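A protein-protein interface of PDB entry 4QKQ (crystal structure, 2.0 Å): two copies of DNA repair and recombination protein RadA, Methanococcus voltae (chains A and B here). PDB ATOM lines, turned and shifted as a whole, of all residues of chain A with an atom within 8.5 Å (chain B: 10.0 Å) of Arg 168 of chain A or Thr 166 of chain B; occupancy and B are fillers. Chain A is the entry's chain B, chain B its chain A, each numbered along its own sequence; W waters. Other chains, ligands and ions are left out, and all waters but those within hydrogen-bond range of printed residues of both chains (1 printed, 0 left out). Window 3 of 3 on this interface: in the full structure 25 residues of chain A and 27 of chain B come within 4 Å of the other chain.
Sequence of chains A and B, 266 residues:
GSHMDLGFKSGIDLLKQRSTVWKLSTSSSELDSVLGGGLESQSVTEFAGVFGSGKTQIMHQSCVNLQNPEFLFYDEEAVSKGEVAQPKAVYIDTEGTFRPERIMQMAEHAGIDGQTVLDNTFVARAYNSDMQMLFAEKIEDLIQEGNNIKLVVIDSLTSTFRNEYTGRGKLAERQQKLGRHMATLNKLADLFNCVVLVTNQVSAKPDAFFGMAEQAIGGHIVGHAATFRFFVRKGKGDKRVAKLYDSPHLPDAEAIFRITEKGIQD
OH of Tyr 165 of chain B lies within hydrogen-bond range of OE1 of Glu 173 of chain B (3.4 Å). The side-chain amino group (NZ) of Lys 170 of chain B lies within salt-bridge range of the side-chain carboxylate (OE2) of Glu 173 of chain B, at 3.6 Å. O of Ala 172 of chain A is in hydrogen-bond range of NE2 of Gln 176 of chain A (3.2 Å). The guanidinium group (NH1) of Arg 174 of chain A is in hydrogen-bond range of the side-chain amide oxygen (OE1) of Gln 175 of chain A (2.8 Å). NE2 of Gln 175 of chain A sits at hydrogen-bond distance from O of Gly 218 of chain A, at 2.9 Å.
Arg 168 of chain A touches Thr 166 of chain B, but with the chains exchanged Thr 166 of chain A does not touch Arg 168 of chain B (14.1 Å). Leu 171 of chain A touches Thr 166 of chain B, but with the chains exchanged Thr 166 of chain A does not touch Leu 171 of chain B (16.0 Å). Ala 172 of chain A touches Lys 170 of chain B, but with the chains exchanged Lys 170 of chain A does not touch Ala 172 of chain B (13.3 Å). Of the 9 pairs that touch across the chains among the printed residues, none has its exchanged pair printed and touching as well.
Hydrophobic or aromatic side chains of chain B within 4 Å of the printed part of chain A: Tyr 165. Of the 15 printed residues of chain A, 6 touch a printed residue of chain B. Printed residues of chain A that touch a printed residue of chain B: Arg 168, Leu 171, Ala 172, Gln 175, Gln 176 and Ile 221. Among the printed residues, no Asp or Glu carboxylate lies within 4 Å of a Lys or Arg side-chain nitrogen of the other chain.
CD2 of Leu 171 of chain A touches OG1 of Thr 166 of chain B (3.1 Å). CA of Ala 172 of chain A touches O of Glu 164 of chain B (3.4 Å). Lys 170 of chain B touches Ala 172 of chain A. O of Asn 163 of chain B touches CG of Gln 175 of chain A, 3.7 Å away. CA of Glu 164 of chain B touches CB of Gln 175 of chain A, at 3.99 Å. CG of Gln 176 of chain A touches CB of Glu 164 of chain B, 3.9 Å away. Tyr 165 of chain B touches Gln 176 of chain A (CE1 to NE2, 3.5 Å). Asn 163 of chain B touches Ile 221 of chain A.
Water W1 lies within hydrogen-bond range of the backbone carbonyl oxygen of Asn 163 of chain B (2.8 Å), the side-chain amide nitrogen of Gln 175 of chain A (2.8 Å) and the backbone NH of Ile 221 of chain A (3.0 Å).
Of chain B, only Thr 166 comes within 4 Å of Arg 168 of chain A. Of chain A, only Arg 168 (3.0 Å) and Leu 171 (3.1 Å) come within 4 Å of Thr 166 of chain B. No residue of chain B comes within 4 Å of Gly 169 of chain A. No residue of chain A comes within 4 Å of Gly 167 of chain B. Of the printed residues of chain B, Gln 175 of chain A touches Asn 163 (3.7 Å) and Glu 164 (3.99 Å). Of the printed residues of chain A, Tyr 165 of chain B touches Gln 176. Of the printed residues of chain B, Gln 176 of chain A touches Glu 164 and Tyr 165. Of the printed residues of chain B, Ala 172 of chain A touches Glu 164 and Lys 170. Of the printed residues of chain B, Ile 221 of chain A touches Asn 163 (3.8 Å). The nearest residue of chain B that does not touch Arg 168 of chain A is Gly 167 of chain B (4.2 Å). The nearest printed residue of chain A that does not touch Lys 170 of chain B is Gln 176 of chain A (5.3 Å).
The side-chain hydroxyl (OG1) of Thr 166 of chain B lies close to the guanidinium group (NH2) of Arg 168 of chain A, at 3.3 Å.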
ATOM      1  N   TYR A 165     -28.737 -14.487 -21.059  1.00  0.00           N
ATOM      2  CA  TYR A 165     -29.216 -13.121 -20.952  1.00  0.00           C
ATOM      3  C   TYR A 165     -30.714 -13.016 -21.073  1.00  0.00           C
ATOM      4  O   TYR A 165     -31.254 -12.880 -22.165  1.00  0.00           O
ATOM      5  CB  TYR A 165     -28.569 -12.257 -22.020  1.00  0.00           C
ATOM      6  CG  TYR A 165     -27.083 -12.186 -21.877  1.00  0.00           C
ATOM      7  CD1 TYR A 165     -26.485 -11.234 -21.049  1.00  0.00           C
ATOM      8  CD2 TYR A 165     -26.269 -13.090 -22.547  1.00  0.00           C
ATOM      9  CE1 TYR A 165     -25.103 -11.188 -20.901  1.00  0.00           C
ATOM     10  CE2 TYR A 165     -24.891 -13.058 -22.401  1.00  0.00           C
ATOM     11  CZ  TYR A 165     -24.312 -12.103 -21.576  1.00  0.00           C
ATOM     12  OH  TYR A 165     -22.944 -12.099 -21.416  1.00  0.00           O
ATOM     13  N   THR A 166     -31.383 -13.098 -19.936  1.00  0.00           N
ATOM     14  CA  THR A 166     -32.825 -12.973 -19.891  1.00  0.00           C
ATOM     15  C   THR A 166     -33.084 -11.547 -19.394  1.00  0.00           C
ATOM     16  O   THR A 166     -32.301 -11.004 -18.600  1.00  0.00           O
ATOM     17  CB  THR A 166     -33.427 -14.012 -18.927  1.00  0.00           C
ATOM     18  OG1 THR A 166     -32.817 -13.881 -17.635  1.00  0.00           O
ATOM     19  CG2 THR A 166     -33.175 -15.427 -19.458  1.00  0.00           C
ATOM     20  N   GLY A 167     -34.155 -10.932 -19.888  1.00  0.00           N
ATOM     21  CA  GLY A 167     -34.475  -9.575 -19.480  1.00  0.00           C
ATOM     22  C   GLY A 167     -33.786  -8.518 -20.332  1.00  0.00           C
ATOM     23  O   GLY A 167     -32.646  -8.704 -20.772  1.00  0.00           O
ATOM     24  N   ARG A 168     -34.478  -7.405 -20.554  1.00  0.00           N
ATOM     25  CA  ARG A 168     -33.965  -6.299 -21.358  1.00  0.00           C
ATOM     26  C   ARG A 168     -32.818  -5.527 -20.709  1.00  0.00           C
ATOM     27  O   ARG A 168     -32.203  -4.672 -21.350  1.00  0.00           O
ATOM     28  CB  ARG A 168     -35.104  -5.329 -21.685  1.00  0.00           C
ATOM     29  CG  ARG A 168     -35.841  -5.621 -22.986  1.00  0.00           C
ATOM     30  CD  ARG A 168     -35.168  -4.925 -24.170  1.00  0.00           C
ATOM     31  NE  ARG A 168     -35.863  -5.164 -25.436  1.00  0.00           N
ATOM     32  CZ  ARG A 168     -35.602  -4.515 -26.569  1.00  0.00           C
ATOM     33  NH1 ARG A 168     -36.280  -4.800 -27.673  1.00  0.00           N
ATOM     34  NH2 ARG A 168     -34.667  -3.572 -26.595  1.00  0.00           N
ATOM     35  N   GLY A 169     -32.520  -5.825 -19.448  1.00  0.00           N
ATOM     36  CA  GLY A 169     -31.452  -5.116 -18.766  1.00  0.00           C
ATOM     37  C   GLY A 169     -30.059  -5.614 -19.089  1.00  0.00           C
ATOM     38  O   GLY A 169     -29.057  -5.008 -18.699  1.00  0.00           O
ATOM     39  N   LYS A 170     -29.989  -6.722 -19.812  1.00  0.00           N
ATOM     40  CA  LYS A 170     -28.710  -7.309 -20.171  1.00  0.00           C
ATOM     41  C   LYS A 170     -28.583  -7.435 -21.678  1.00  0.00           C
ATOM     42  O   LYS A 170     -27.519  -7.772 -22.196  1.00  0.00           O
ATOM     43  CB  LYS A 170     -28.584  -8.689 -19.522  1.00  0.00           C
ATOM     44  CG  LYS A 170     -27.501  -8.776 -18.470  1.00  0.00           C
ATOM     45  CD  LYS A 170     -27.738  -7.799 -17.333  1.00  0.00           C
ATOM     46  CE  LYS A 170     -26.617  -7.886 -16.308  1.00  0.00           C
ATOM     47  NZ  LYS A 170     -25.276  -7.693 -16.941  1.00  0.00           N
ATOM     48  N   LEU A 171     -29.681  -7.146 -22.367  1.00  0.00           N
ATOM     49  CA  LEU A 171     -29.744  -7.244 -23.813  1.00  0.00           C
ATOM     50  C   LEU A 171     -28.569  -6.593 -24.527  1.00  0.00           C
ATOM     51  O   LEU A 171     -28.069  -7.123 -25.517  1.00  0.00           O
ATOM     52  CB  LEU A 171     -31.059  -6.652 -24.312  1.00  0.00           C
ATOM     53  CG  LEU A 171     -31.348  -6.767 -25.807  1.00  0.00           C
ATOM     54  CD1 LEU A 171     -31.253  -8.230 -26.273  1.00  0.00           C
ATOM     55  CD2 LEU A 171     -32.734  -6.216 -26.072  1.00  0.00           C
ATOM     56  N   ALA A 172     -28.112  -5.452 -24.024  1.00  0.00           N
ATOM     57  CA  ALA A 172     -26.987  -4.767 -24.639  1.00  0.00           C
ATOM     58  C   ALA A 172     -25.737  -5.630 -24.520  1.00  0.00           C
ATOM     59  O   ALA A 172     -24.964  -5.773 -25.466  1.00  0.00           O
ATOM     60  CB  ALA A 172     -26.757  -3.410 -23.963  1.00  0.00           C
ATOM     61  N   GLU A 173     -25.521  -6.202 -23.347  1.00  0.00           N
ATOM     62  CA  GLU A 173     -24.347  -7.046 -23.165  1.00  0.00           C
ATOM     63  C   GLU A 173     -24.458  -8.293 -24.060  1.00  0.00           C
ATOM     64  O   GLU A 173     -23.482  -8.757 -24.637  1.00  0.00           O
ATOM     65  CB  GLU A 173     -24.226  -7.463 -21.703  1.00  0.00           C
ATOM     66  CG  GLU A 173     -22.996  -8.314 -21.409  1.00  0.00           C
ATOM     67  CD  GLU A 173     -22.950  -8.789 -19.960  1.00  0.00           C
ATOM     68  OE1 GLU A 173     -22.035  -9.571 -19.624  1.00  0.00           O
ATOM     69  OE2 GLU A 173     -23.826  -8.381 -19.161  1.00  0.00           O
ATOM     70  N   ARG A 174     -25.660  -8.829 -24.170  1.00  0.00           N
ATOM     71  CA  ARG A 174     -25.857 -10.002 -25.003  1.00  0.00           C
ATOM     72  C   ARG A 174     -25.540  -9.641 -26.468  1.00  0.00           C
ATOM     73  O   ARG A 174     -24.795 -10.349 -27.134  1.00  0.00           O
ATOM     74  CB  ARG A 174     -27.294 -10.496 -24.852  1.00  0.00           C
ATOM     75  CG  ARG A 174     -27.641 -11.727 -25.669  1.00  0.00           C
ATOM     76  CD  ARG A 174     -28.573 -11.339 -26.783  1.00  0.00           C
ATOM     77  NE  ARG A 174     -29.873 -11.950 -26.607  1.00  0.00           N
ATOM     78  CZ  ARG A 174     -30.895 -11.794 -27.440  1.00  0.00           C
ATOM     79  NH1 ARG A 174     -30.778 -11.033 -28.520  1.00  0.00           N
ATOM     80  NH2 ARG A 174     -32.034 -12.425 -27.200  1.00  0.00           N
ATOM     81  N   GLN A 175     -26.086  -8.528 -26.958  1.00  0.00           N
ATOM     82  CA  GLN A 175     -25.855  -8.107 -28.340  1.00  0.00           C
ATOM     83  C   GLN A 175     -24.388  -7.905 -28.668  1.00  0.00           C
ATOM     84  O   GLN A 175     -23.915  -8.280 -29.752  1.00  0.00           O
ATOM     85  CB  GLN A 175     -26.630  -6.826 -28.657  1.00  0.00           C
ATOM     86  CG  GLN A 175     -28.119  -7.006 -28.684  1.00  0.00           C
ATOM     87  CD  GLN A 175     -28.550  -8.254 -29.461  1.00  0.00           C
ATOM     88  OE1 GLN A 175     -28.578  -9.358 -28.914  1.00  0.00           O
ATOM     89  NE2 GLN A 175     -28.883  -8.080 -30.740  1.00  0.00           N
ATOM     90  N   GLN A 176     -23.650  -7.341 -27.727  1.00  0.00           N
ATOM     91  CA  GLN A 176     -22.234  -7.116 -27.947  1.00  0.00           C
ATOM     92  C   GLN A 176     -21.432  -8.418 -27.945  1.00  0.00           C
ATOM     93  O   GLN A 176     -20.472  -8.561 -28.697  1.00  0.00           O
ATOM     94  CB  GLN A 176     -21.683  -6.181 -26.878  1.00  0.00           C
ATOM     95  CG  GLN A 176     -22.265  -4.768 -26.940  1.00  0.00           C
ATOM     96  CD  GLN A 176     -21.899  -3.955 -25.710  1.00  0.00           C
ATOM     97  OE1 GLN A 176     -20.729  -3.885 -25.323  1.00  0.00           O
ATOM     98  NE2 GLN A 176     -22.900  -3.341 -25.086  1.00  0.00           N
ATOM     99  N   GLY A 218     -31.494 -12.633 -32.308  1.00  0.00           N
ATOM    100  CA  GLY A 218     -30.216 -11.947 -32.307  1.00  0.00           C
ATOM    101  C   GLY A 218     -30.290 -10.611 -33.022  1.00  0.00           C
ATOM    102  O   GLY A 218     -29.329  -9.841 -33.020  1.00  0.00           O
ATOM    103  N   GLY A 219     -31.426 -10.351 -33.657  1.00  0.00           N
ATOM    104  CA  GLY A 219     -31.628  -9.101 -34.363  1.00  0.00           C
ATOM    105  C   GLY A 219     -30.644  -8.763 -35.473  1.00  0.00           C
ATOM    106  O   GLY A 219     -30.067  -9.642 -36.113  1.00  0.00           O
ATOM    107  N   ILE A 221     -27.700  -7.388 -35.251  1.00  0.00           N
ATOM    108  CA  ILE A 221     -26.313  -7.667 -34.928  1.00  0.00           C
ATOM    109  C   ILE A 221     -25.880  -8.954 -35.644  1.00  0.00           C
ATOM    110  O   ILE A 221     -24.745  -9.071 -36.127  1.00  0.00           O
ATOM    111  CB  ILE A 221     -26.124  -7.785 -33.388  1.00  0.00           C
ATOM    112  CG1 ILE A 221     -25.148  -6.716 -32.928  1.00  0.00           C
ATOM    113  CG2 ILE A 221     -25.603  -9.144 -32.988  1.00  0.00           C
ATOM    114  CD1 ILE A 221     -23.862  -6.742 -33.655  1.00  0.00           C
ATOM    115  N   SER B 159     -24.930   2.348 -37.354  1.00  0.00           N
ATOM    116  CA  SER B 159     -25.573   1.040 -37.471  1.00  0.00           C
ATOM    117  C   SER B 159     -25.198   0.100 -36.315  1.00  0.00           C
ATOM    118  O   SER B 159     -26.068  -0.411 -35.600  1.00  0.00           O
ATOM    119  CB  SER B 159     -25.181   0.408 -38.810  1.00  0.00           C
ATOM    120  OG  SER B 159     -25.893  -0.783 -39.031  1.00  0.00           O
ATOM    121  N   THR B 160     -23.906  -0.113 -36.124  1.00  0.00           N
ATOM    122  CA  THR B 160     -23.420  -1.004 -35.069  1.00  0.00           C
ATOM    123  C   THR B 160     -23.823  -0.551 -33.652  1.00  0.00           C
ATOM    124  O   THR B 160     -24.314  -1.352 -32.841  1.00  0.00           O
ATOM    125  CB  THR B 160     -21.880  -1.168 -35.165  1.00  0.00           C
ATOM    126  OG1 THR B 160     -21.233   0.099 -34.962  1.00  0.00           O
ATOM    127  CG2 THR B 160     -21.492  -1.712 -36.545  1.00  0.00           C
ATOM    128  N   PHE B 161     -23.628   0.727 -33.354  1.00  0.00           N
ATOM    129  CA  PHE B 161     -23.992   1.251 -32.044  1.00  0.00           C
ATOM    130  C   PHE B 161     -25.468   1.034 -31.764  1.00  0.00           C
ATOM    131  O   PHE B 161     -25.862   0.637 -30.668  1.00  0.00           O
ATOM    132  CB  PHE B 161     -23.680   2.739 -31.960  1.00  0.00           C
ATOM    133  CG  PHE B 161     -22.233   3.047 -32.103  1.00  0.00           C
ATOM    134  CD1 PHE B 161     -21.680   3.298 -33.357  1.00  0.00           C
ATOM    135  CD2 PHE B 161     -21.411   3.097 -30.984  1.00  0.00           C
ATOM    136  CE1 PHE B 161     -20.331   3.599 -33.482  1.00  0.00           C
ATOM    137  CE2 PHE B 161     -20.060   3.400 -31.108  1.00  0.00           C
ATOM    138  CZ  PHE B 161     -19.522   3.652 -32.360  1.00  0.00           C
ATOM    139  N   ARG B 162     -26.283   1.289 -32.772  1.00  0.00           N
ATOM    140  CA  ARG B 162     -27.715   1.121 -32.649  1.00  0.00           C
ATOM    141  C   ARG B 162     -28.085  -0.351 -32.467  1.00  0.00           C
ATOM    142  O   ARG B 162     -29.034  -0.660 -31.751  1.00  0.00           O
ATOM    143  CB  ARG B 162     -28.406   1.701 -33.883  1.00  0.00           C
ATOM    144  CG  ARG B 162     -29.888   1.844 -33.726  1.00  0.00           C
ATOM    145  CD  ARG B 162     -30.518   2.748 -34.786  1.00  0.00           C
ATOM    146  NE  ARG B 162     -31.975   2.810 -34.610  1.00  0.00           N
ATOM    147  CZ  ARG B 162     -32.589   3.267 -33.517  1.00  0.00           C
ATOM    148  NH1 ARG B 162     -31.882   3.721 -32.487  1.00  0.00           N
ATOM    149  NH2 ARG B 162     -33.916   3.251 -33.445  1.00  0.00           N
ATOM    150  N   ASN B 163     -27.334  -1.256 -33.100  1.00  0.00           N
ATOM    151  CA  ASN B 163     -27.608  -2.698 -32.991  1.00  0.00           C
ATOM    152  C   ASN B 163     -27.177  -3.275 -31.649  1.00  0.00           C
ATOM    153  O   ASN B 163     -27.730  -4.259 -31.191  1.00  0.00           O
ATOM    154  CB  ASN B 163     -26.885  -3.494 -34.092  1.00  0.00           C
ATOM    155  CG  ASN B 163     -27.583  -3.419 -35.432  1.00  0.00           C
ATOM    156  OD1 ASN B 163     -28.748  -3.025 -35.520  1.00  0.00           O
ATOM    157  ND2 ASN B 163     -26.877  -3.820 -36.489  1.00  0.00           N
ATOM    158  N   GLU B 164     -26.187  -2.654 -31.028  1.00  0.00           N
ATOM    159  CA  GLU B 164     -25.653  -3.117 -29.759  1.00  0.00           C
ATOM    160  C   GLU B 164     -26.282  -2.503 -28.515  1.00  0.00           C
ATOM    161  O   GLU B 164     -26.170  -3.052 -27.417  1.00  0.00           O
ATOM    162  CB  GLU B 164     -24.149  -2.850 -29.718  1.00  0.00           C
ATOM    163  CG  GLU B 164     -23.352  -3.653 -30.719  1.00  0.00           C
ATOM    164  CD  GLU B 164     -21.916  -3.187 -30.825  1.00  0.00           C
ATOM    165  OE1 GLU B 164     -21.172  -3.759 -31.646  1.00  0.00           O
ATOM    166  OE2 GLU B 164     -21.533  -2.247 -30.088  1.00  0.00           O
ATOM    167  N   TYR B 165     -26.933  -1.363 -28.679  1.00  0.00           N
ATOM    168  CA  TYR B 165     -27.520  -0.685 -27.536  1.00  0.00           C
ATOM    169  C   TYR B 165     -29.014  -0.476 -27.606  1.00  0.00           C
ATOM    170  O   TYR B 165     -29.517   0.397 -28.308  1.00  0.00           O
ATOM    171  CB  TYR B 165     -26.816   0.653 -27.320  1.00  0.00           C
ATOM    172  CG  TYR B 165     -25.381   0.494 -26.888  1.00  0.00           C
ATOM    173  CD1 TYR B 165     -25.058   0.268 -25.552  1.00  0.00           C
ATOM    174  CD2 TYR B 165     -24.345   0.538 -27.817  1.00  0.00           C
ATOM    175  CE1 TYR B 165     -23.734   0.087 -25.150  1.00  0.00           C
ATOM    176  CE2 TYR B 165     -23.013   0.361 -27.427  1.00  0.00           C
ATOM    177  CZ  TYR B 165     -22.721   0.132 -26.085  1.00  0.00           C
ATOM    178  OH  TYR B 165     -21.418  -0.075 -25.683  1.00  0.00           O
ATOM    179  N   THR B 166     -29.717  -1.309 -26.860  1.00  0.00           N
ATOM    180  CA  THR B 166     -31.160  -1.237 -26.763  1.00  0.00           C
ATOM    181  C   THR B 166     -31.366  -0.771 -25.324  1.00  0.00           C
ATOM    182  O   THR B 166     -30.450  -0.874 -24.495  1.00  0.00           O
ATOM    183  CB  THR B 166     -31.793  -2.627 -26.943  1.00  0.00           C
ATOM    184  OG1 THR B 166     -31.405  -3.462 -25.843  1.00  0.00           O
ATOM    185  CG2 THR B 166     -31.312  -3.271 -28.248  1.00  0.00           C
ATOM    186  N   GLY B 167     -32.548  -0.247 -25.030  1.00  0.00           N
ATOM    187  CA  GLY B 167     -32.818   0.212 -23.683  1.00  0.00           C
ATOM    188  C   GLY B 167     -32.195   1.554 -23.340  1.00  0.00           C
ATOM    189  O   GLY B 167     -30.996   1.778 -23.528  1.00  0.00           O
ATOM    190  N   ARG B 168     -33.030   2.454 -22.833  1.00  0.00           N
ATOM    191  CA  ARG B 168     -32.592   3.781 -22.435  1.00  0.00           C
ATOM    192  C   ARG B 168     -31.579   3.679 -21.293  1.00  0.00           C
ATOM    193  O   ARG B 168     -30.882   4.646 -20.976  1.00  0.00           O
ATOM    194  CB  ARG B 168     -33.804   4.604 -21.990  1.00  0.00           C
ATOM    195  CG  ARG B 168     -34.685   5.086 -23.133  1.00  0.00           C
ATOM    196  CD  ARG B 168     -34.087   6.328 -23.775  1.00  0.00           C
ATOM    197  NE  ARG B 168     -34.823   6.774 -24.954  1.00  0.00           N
ATOM    198  CZ  ARG B 168     -34.660   7.966 -25.525  1.00  0.00           C
ATOM    199  NH1 ARG B 168     -35.367   8.292 -26.601  1.00  0.00           N
ATOM    200  NH2 ARG B 168     -33.798   8.838 -25.010  1.00  0.00           N
ATOM    201  N   GLY B 169     -31.501   2.499 -20.685  1.00  0.00           N
ATOM    202  CA  GLY B 169     -30.584   2.290 -19.576  1.00  0.00           C
ATOM    203  C   GLY B 169     -29.177   1.958 -20.016  1.00  0.00           C
ATOM    204  O   GLY B 169     -28.300   1.657 -19.203  1.00  0.00           O
ATOM    205  N   LYS B 170     -28.953   2.012 -21.319  1.00  0.00           N
ATOM    206  CA  LYS B 170     -27.640   1.714 -21.856  1.00  0.00           C
ATOM    207  C   LYS B 170     -27.222   2.863 -22.752  1.00  0.00           C
ATOM    208  O   LYS B 170     -26.076   2.929 -23.202  1.00  0.00           O
ATOM    209  CB  LYS B 170     -27.692   0.407 -22.656  1.00  0.00           C
ATOM    210  CG  LYS B 170     -26.524  -0.496 -22.368  1.00  0.00           C
ATOM    211  CD  LYS B 170     -26.462  -0.787 -20.884  1.00  0.00           C
ATOM    212  CE  LYS B 170     -25.090  -1.264 -20.472  1.00  0.00           C
ATOM    213  NZ  LYS B 170     -24.936  -1.199 -18.990  1.00  0.00           N
ATOM    214  N   LEU B 171     -28.168   3.767 -22.985  1.00  0.00           N
ATOM    215  CA  LEU B 171     -27.970   4.926 -23.842  1.00  0.00           C
ATOM    216  C   LEU B 171     -26.777   5.795 -23.466  1.00  0.00           C
ATOM    217  O   LEU B 171     -26.127   6.368 -24.337  1.00  0.00           O
ATOM    218  CB  LEU B 171     -29.244   5.769 -23.865  1.00  0.00           C
ATOM    219  CG  LEU B 171     -29.294   6.873 -24.924  1.00  0.00           C
ATOM    220  CD1 LEU B 171     -28.905   6.303 -26.289  1.00  0.00           C
ATOM    221  CD2 LEU B 171     -30.690   7.469 -24.975  1.00  0.00           C
ATOM    222  N   ALA B 172     -26.477   5.886 -22.178  1.00  0.00           N
ATOM    223  CA  ALA B 172     -25.354   6.696 -21.728  1.00  0.00           C
ATOM    224  C   ALA B 172     -24.040   6.125 -22.240  1.00  0.00           C
ATOM    225  O   ALA B 172     -23.174   6.856 -22.738  1.00  0.00           O
ATOM    226  CB  ALA B 172     -25.337   6.771 -20.208  1.00  0.00           C
ATOM    227  N   GLU B 173     -23.887   4.812 -22.115  1.00  0.00           N
ATOM    228  CA  GLU B 173     -22.676   4.151 -22.580  1.00  0.00           C
ATOM    229  C   GLU B 173     -22.539   4.251 -24.122  1.00  0.00           C
ATOM    230  O   GLU B 173     -21.446   4.436 -24.660  1.00  0.00           O
ATOM    231  CB  GLU B 173     -22.702   2.688 -22.140  1.00  0.00           C
ATOM    232  CG  GLU B 173     -21.443   1.896 -22.480  1.00  0.00           C
ATOM    233  CD  GLU B 173     -21.525   0.452 -21.985  1.00  0.00           C
ATOM    234  OE1 GLU B 173     -20.641  -0.360 -22.343  1.00  0.00           O
ATOM    235  OE2 GLU B 173     -22.478   0.135 -21.233  1.00  0.00           O
ATOM    236  N   ARG B 174     -23.655   4.124 -24.821  1.00  0.00           N
ATOM    237  CA  ARG B 174     -23.651   4.209 -26.270  1.00  0.00           C
ATOM    238  C   ARG B 174     -23.168   5.607 -26.702  1.00  0.00           C
ATOM    239  O   ARG B 174     -22.361   5.724 -27.619  1.00  0.00           O
ATOM    240  CB  ARG B 174     -25.063   3.924 -26.795  1.00  0.00           C
ATOM    241  CG  ARG B 174     -25.242   4.004 -28.299  1.00  0.00           C
ATOM    242  CD  ARG B 174     -26.018   5.249 -28.660  1.00  0.00           C
ATOM    243  NE  ARG B 174     -27.268   4.928 -29.314  1.00  0.00           N
ATOM    244  CZ  ARG B 174     -28.162   5.818 -29.731  1.00  0.00           C
ATOM    245  NH1 ARG B 174     -27.957   7.118 -29.564  1.00  0.00           N
ATOM    246  NH2 ARG B 174     -29.267   5.399 -30.328  1.00  0.00           N
HETATM  247  O   HOH W   1     -28.966  -6.168 -32.763  1.00  0.00           O
